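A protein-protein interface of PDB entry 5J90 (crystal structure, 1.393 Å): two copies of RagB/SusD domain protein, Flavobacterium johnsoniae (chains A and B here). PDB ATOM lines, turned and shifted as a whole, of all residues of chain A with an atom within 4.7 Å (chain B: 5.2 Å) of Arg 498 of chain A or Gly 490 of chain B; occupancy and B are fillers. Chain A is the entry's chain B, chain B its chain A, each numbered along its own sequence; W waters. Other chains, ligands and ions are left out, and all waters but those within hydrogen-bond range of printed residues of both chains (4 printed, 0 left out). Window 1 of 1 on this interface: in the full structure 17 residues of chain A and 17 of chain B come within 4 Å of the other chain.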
ATOM      1  N   PHE A 463       0.020  18.816  23.871  1.00  0.00           N
ATOM      2  CA  PHE A 463      -0.047  19.186  25.285  1.00  0.00           C
ATOM      3  C   PHE A 463      -0.757  18.150  26.152  1.00  0.00           C
ATOM      4  O   PHE A 463      -0.628  18.179  27.372  1.00  0.00           O
ATOM      5  CB  PHE A 463      -0.621  20.607  25.450  1.00  0.00           C
ATOM      6  CG  PHE A 463       0.227  21.643  24.773  1.00  0.00           C
ATOM      7  CD1 PHE A 463       1.392  22.087  25.376  1.00  0.00           C
ATOM      8  CD2 PHE A 463      -0.086  22.078  23.497  1.00  0.00           C
ATOM      9  CE1 PHE A 463       2.211  23.000  24.738  1.00  0.00           C
ATOM     10  CE2 PHE A 463       0.736  22.987  22.852  1.00  0.00           C
ATOM     11  CZ  PHE A 463       1.877  23.439  23.470  1.00  0.00           C
ATOM     12  N   ARG A 466      -4.938  18.149  30.203  1.00  0.00           N
ATOM     13  CA  ARG A 466      -4.643  19.243  31.132  1.00  0.00           C
ATOM     14  C   ARG A 466      -5.480  19.166  32.411  1.00  0.00           C
ATOM     15  O   ARG A 466      -5.116  19.761  33.428  1.00  0.00           O
ATOM     16  CB  ARG A 466      -4.834  20.616  30.464  1.00  0.00           C
ATOM     17  CG  ARG A 466      -4.116  20.793  29.114  1.00  0.00           C
ATOM     18  CD  ARG A 466      -2.651  20.343  29.130  1.00  0.00           C
ATOM     19  NE  ARG A 466      -1.789  21.267  29.865  1.00  0.00           N
ATOM     20  CZ  ARG A 466      -0.466  21.289  29.773  1.00  0.00           C
ATOM     21  NH1 ARG A 466       0.177  20.450  28.970  1.00  0.00           N
ATOM     22  NH2 ARG A 466       0.227  22.175  30.474  1.00  0.00           N
ATOM     23  N   GLY A 496      -9.024  19.557  27.750  1.00  0.00           N
ATOM     24  CA  GLY A 496      -8.103  20.483  27.107  1.00  0.00           C
ATOM     25  C   GLY A 496      -8.030  21.856  27.754  1.00  0.00           C
ATOM     26  O   GLY A 496      -7.065  22.595  27.563  1.00  0.00           O
ATOM     27  N   THR A 497      -9.056  22.201  28.523  1.00  0.00           N
ATOM     28  CA  THR A 497      -9.133  23.485  29.199  1.00  0.00           C
ATOM     29  C   THR A 497      -8.157  23.508  30.370  1.00  0.00           C
ATOM     30  O   THR A 497      -8.125  22.584  31.183  1.00  0.00           O
ATOM     31  CB  THR A 497     -10.557  23.721  29.691  1.00  0.00           C
ATOM     32  OG1 THR A 497     -11.421  23.774  28.550  1.00  0.00           O
ATOM     33  CG2 THR A 497     -10.661  25.021  30.468  1.00  0.00           C
ATOM     34  N   ARG A 498      -7.341  24.558  30.441  1.00  0.00           N
ATOM     35  CA  ARG A 498      -6.305  24.651  31.462  1.00  0.00           C
ATOM     36  C   ARG A 498      -6.847  25.143  32.796  1.00  0.00           C
ATOM     37  O   ARG A 498      -7.627  26.099  32.843  1.00  0.00           O
ATOM     38  CB  ARG A 498      -5.195  25.596  30.988  1.00  0.00           C
ATOM     39  CG  ARG A 498      -4.352  24.981  29.896  1.00  0.00           C
ATOM     40  CD  ARG A 498      -3.533  26.019  29.141  1.00  0.00           C
ATOM     41  NE  ARG A 498      -2.663  25.332  28.195  1.00  0.00           N
ATOM     42  CZ  ARG A 498      -1.423  24.945  28.452  1.00  0.00           C
ATOM     43  NH1 ARG A 498      -0.861  25.233  29.619  1.00  0.00           N
ATOM     44  NH2 ARG A 498      -0.730  24.277  27.538  1.00  0.00           N
ATOM     45  N   VAL A 499      -6.436  24.487  33.883  1.00  0.00           N
ATOM     46  CA  VAL A 499      -6.746  25.001  35.216  1.00  0.00           C
ATOM     47  C   VAL A 499      -5.954  26.285  35.468  1.00  0.00           C
ATOM     48  O   VAL A 499      -4.986  26.573  34.755  1.00  0.00           O
ATOM     49  CB  VAL A 499      -6.484  23.966  36.346  1.00  0.00           C
ATOM     50  CG1 VAL A 499      -7.236  22.658  36.059  1.00  0.00           C
ATOM     51  CG2 VAL A 499      -4.992  23.701  36.530  1.00  0.00           C
ATOM     52  N   TRP A 500      -6.374  27.037  36.483  1.00  0.00           N
ATOM     53  CA  TRP A 500      -5.807  28.340  36.805  1.00  0.00           C
ATOM     54  C   TRP A 500      -4.270  28.388  36.845  1.00  0.00           C
ATOM     55  O   TRP A 500      -3.666  29.280  36.242  1.00  0.00           O
ATOM     56  CB  TRP A 500      -6.426  28.819  38.125  1.00  0.00           C
ATOM     57  CG  TRP A 500      -5.741  29.977  38.815  1.00  0.00           C
ATOM     58  CD1 TRP A 500      -5.829  31.306  38.504  1.00  0.00           C
ATOM     59  CD2 TRP A 500      -4.891  29.887  39.965  1.00  0.00           C
ATOM     60  NE1 TRP A 500      -5.068  32.051  39.388  1.00  0.00           N
ATOM     61  CE2 TRP A 500      -4.492  31.201  40.297  1.00  0.00           C
ATOM     62  CE3 TRP A 500      -4.429  28.820  40.748  1.00  0.00           C
ATOM     63  CZ2 TRP A 500      -3.641  31.474  41.386  1.00  0.00           C
ATOM     64  CZ3 TRP A 500      -3.596  29.092  41.829  1.00  0.00           C
ATOM     65  CH2 TRP A 500      -3.213  30.410  42.135  1.00  0.00           C
ATOM     66  N   ASP A 502      -2.165  26.407  35.460  1.00  0.00           N
ATOM     67  CA  ASP A 502      -1.603  25.859  34.226  1.00  0.00           C
ATOM     68  C   ASP A 502      -1.741  26.848  33.056  1.00  0.00           C
ATOM     69  O   ASP A 502      -2.152  26.500  31.947  1.00  0.00           O
ATOM     70  CB  ASP A 502      -2.326  24.541  33.915  1.00  0.00           C
ATOM     71  CG  ASP A 502      -1.667  23.732  32.815  1.00  0.00           C
ATOM     72  OD1 ASP A 502      -0.458  23.897  32.570  1.00  0.00           O
ATOM     73  OD2 ASP A 502      -2.382  22.907  32.203  1.00  0.00           O
ATOM     74  N   VAL A 503      -1.395  28.097  33.315  1.00  0.00           N
ATOM     75  CA  VAL A 503      -1.553  29.128  32.309  1.00  0.00           C
ATOM     76  C   VAL A 503      -0.617  28.874  31.120  1.00  0.00           C
ATOM     77  O   VAL A 503       0.499  28.361  31.264  1.00  0.00           O
ATOM     78  CB  VAL A 503      -1.331  30.512  32.944  1.00  0.00           C
ATOM     79  CG1 VAL A 503       0.052  30.592  33.531  1.00  0.00           C
ATOM     80  CG2 VAL A 503      -1.593  31.633  31.940  1.00  0.00           C
ATOM     81  N   ASN A 504      -1.108  29.213  29.930  1.00  0.00           N
ATOM     82  CA  ASN A 504      -0.283  29.131  28.736  1.00  0.00           C
ATOM     83  C   ASN A 504       0.720  30.281  28.725  1.00  0.00           C
ATOM     84  O   ASN A 504       0.460  31.366  28.195  1.00  0.00           O
ATOM     85  CB  ASN A 504      -1.121  29.165  27.463  1.00  0.00           C
ATOM     86  CG  ASN A 504      -0.267  28.998  26.232  1.00  0.00           C
ATOM     87  OD1 ASN A 504       0.503  28.048  26.138  1.00  0.00           O
ATOM     88  ND2 ASN A 504      -0.371  29.923  25.295  1.00  0.00           N
ATOM     89  N   VAL B 486      -0.129  26.982  16.749  1.00  0.00           N
ATOM     90  CA  VAL B 486      -0.883  26.066  17.596  1.00  0.00           C
ATOM     91  C   VAL B 486      -0.053  25.661  18.823  1.00  0.00           C
ATOM     92  O   VAL B 486      -0.566  25.630  19.950  1.00  0.00           O
ATOM     93  CB  VAL B 486      -1.381  24.854  16.787  1.00  0.00           C
ATOM     94  CG1 VAL B 486      -2.085  23.860  17.697  1.00  0.00           C
ATOM     95  CG2 VAL B 486      -2.318  25.321  15.684  1.00  0.00           C
ATOM     96  N   SER B 487       1.235  25.392  18.626  1.00  0.00           N
ATOM     97  CA  SER B 487       2.110  25.084  19.749  1.00  0.00           C
ATOM     98  C   SER B 487       2.082  26.219  20.763  1.00  0.00           C
ATOM     99  O   SER B 487       1.931  25.986  21.963  1.00  0.00           O
ATOM    100  CB  SER B 487       3.546  24.825  19.284  1.00  0.00           C
ATOM    101  OG  SER B 487       3.614  23.680  18.444  1.00  0.00           O
ATOM    102  N   LYS B 488       2.200  27.454  20.280  1.00  0.00           N
ATOM    103  CA  LYS B 488       2.304  28.605  21.169  1.00  0.00           C
ATOM    104  C   LYS B 488       0.953  29.031  21.758  1.00  0.00           C
ATOM    105  O   LYS B 488       0.901  29.843  22.687  1.00  0.00           O
ATOM    106  CB  LYS B 488       3.053  29.747  20.469  1.00  0.00           C
ATOM    107  CG  LYS B 488       4.549  29.415  20.330  1.00  0.00           C
ATOM    108  CD  LYS B 488       5.300  30.283  19.335  1.00  0.00           C
ATOM    109  CE  LYS B 488       6.652  29.652  19.006  1.00  0.00           C
ATOM    110  NZ  LYS B 488       7.563  30.593  18.282  1.00  0.00           N
ATOM    111  N   LEU B 489      -0.125  28.441  21.248  1.00  0.00           N
ATOM    112  CA  LEU B 489      -1.476  28.631  21.778  1.00  0.00           C
ATOM    113  C   LEU B 489      -1.745  27.732  22.994  1.00  0.00           C
ATOM    114  O   LEU B 489      -2.546  28.080  23.862  1.00  0.00           O
ATOM    115  CB  LEU B 489      -2.517  28.356  20.687  1.00  0.00           C
ATOM    116  CG  LEU B 489      -3.989  28.588  21.031  1.00  0.00           C
ATOM    117  CD1 LEU B 489      -4.244  30.077  21.214  1.00  0.00           C
ATOM    118  CD2 LEU B 489      -4.883  28.018  19.925  1.00  0.00           C
ATOM    119  N   GLY B 490      -1.099  26.565  23.045  1.00  0.00           N
ATOM    120  CA  GLY B 490      -1.184  25.697  24.217  1.00  0.00           C
ATOM    121  C   GLY B 490      -2.429  24.840  24.341  1.00  0.00           C
ATOM    122  O   GLY B 490      -2.618  24.156  25.354  1.00  0.00           O
ATOM    123  N   GLY B 491      -3.289  24.870  23.324  1.00  0.00           N
ATOM    124  CA  GLY B 491      -4.532  24.125  23.360  1.00  0.00           C
ATOM    125  C   GLY B 491      -5.183  24.136  21.996  1.00  0.00           C
ATOM    126  O   GLY B 491      -4.585  24.611  21.033  1.00  0.00           O
ATOM    127  N   PRO B 492      -6.410  23.615  21.903  1.00  0.00           N
ATOM    128  CA  PRO B 492      -7.111  23.496  20.618  1.00  0.00           C
ATOM    129  C   PRO B 492      -7.300  24.832  19.900  1.00  0.00           C
ATOM    130  O   PRO B 492      -7.612  25.856  20.514  1.00  0.00           O
ATOM    131  CB  PRO B 492      -8.467  22.893  21.011  1.00  0.00           C
ATOM    132  CG  PRO B 492      -8.172  22.126  22.271  1.00  0.00           C
ATOM    133  CD  PRO B 492      -7.146  22.960  23.000  1.00  0.00           C
HETATM  134  O   HOH W   1      -4.102  26.984  25.990  1.00  0.00           O
HETATM  135  O   HOH W   2       2.424  27.053  24.523  1.00  0.00           O
HETATM  136  O   HOH W   3      -3.113  30.791  24.641  1.00  0.00           O
HETATM  137  O   HOH W   4      -4.808  22.077  26.042  1.00  0.00           O
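No position is printed for both chains.
Of the 6 pairs that touch across the chains among the printed residues, none has its exchanged pair printed and touching as well.
Ser 487 of chain B touches Phe 463 of chain A.
Gly 490 of chain B touches Phe 463 of chain A (CA to CE2, 3.6 Å).
Asn 504 of chain A touches Gly 490 of chain B.
Water W2 lies within hydrogen-bond range of the side-chain amide oxygen (OD1) of Asn 504 of chain A (2.7 Å) and the backbone carbonyl oxygen (O) of Ser 487 of chain B (2.8 Å).
Water W4 bridges O of Gly 496 of chain A (2.8 Å) and O of Gly 490 of chain B (3.1 Å).
Water W1 lies within hydrogen-bond range of O of Leu 489 of chain B (2.9 Å), NE of Arg 498 of chain A (3.1 Å), O of Gly 490 of chain B (3.3 Å) and N of Gly 491 of chain B (3.5 Å).
Water W3 bridges O of Leu 489 of chain B (2.9 Å) and ND2 of Asn 504 of chain A (2.9 Å).
Of the 7 printed residues of chain B, 4 touch a printed residue of chain A.
Printed residues of chain B that touch a printed residue of chain A: Ser 487, Lys 488, Leu 489 and Gly 490.
Along chain B the printed residues that touch a printed residue of chain A span positions 487 to 490.
Hydrophobic or aromatic side chains of chain A that line the printed part of chain B: Phe 463.
Among the printed residues, no Asp or Glu carboxylate lies within 4 Å of a Lys or Arg side-chain nitrogen of the other chain.
The side-chain amide nitrogen (ND2) of Asn 504 of chain A lies within hydrogen-bond range of the backbone carbonyl oxygen (O) of Lys 488 of chain B (2.9 Å).
The backbone carbonyl oxygen (O) of Leu 489 of chain B is in hydrogen-bond range of the side-chain amide nitrogen (ND2) of Asn 504 of chain A, at 3.2 Å.
The backbone carbonyl oxygen (O) of Gly 490 of chain B is in hydrogen-bond range of the guanidinium group (NH2) of Arg 498 of chain A, 2.9 Å away.
Arg 498 of chain A touches just one residue of chain B: Gly 490.
Gly 490 of chain B touches three residues of chain A.
Of the printed residues of chain A, Leu 489 of chain B touches Asn 504 (3.2 Å).
Printed residues of chain B within 4 Å of Phe 463 of chain A: Ser 487 (3.0 Å) and Gly 490 (3.6 Å).
Of the printed residues of chain B, Asn 504 of chain A touches Lys 488 (2.9 Å), Leu 489 (3.2 Å) and Gly 490 (3.5 Å).
Printed residues of chain A within 4 Å of Lys 488 of chain B: Asn 504 (2.9 Å).
Printed residues of chain A within 4 Å of Ser 487 of chain B: Phe 463 (3.0 Å).
Pro 492 of chain B touches none of the printed residues of chain A.
Asp 502 of chain A touches none of the printed residues of chain B.
The nearest residue of chain B that does not touch Arg 498 of chain A is Gly 491 of chain B (4.9 Å).
The nearest printed residue of chain A that does not touch Gly 490 of chain B is Gly 496 of chain A (5.2 Å).
The nearest printed residue of chain A that does not touch Ser 487 of chain B is Asn 504 of chain A (4.9 Å).
NH1 of Arg 466 of chain A sits at hydrogen-bond distance from O of Phe 463 of chain A.
The guanidinium group (NH1) of Arg 498 of chain A is in salt-bridge range of the side-chain carboxylate (OD1) of Asp 502 of chain A (3.3 Å).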
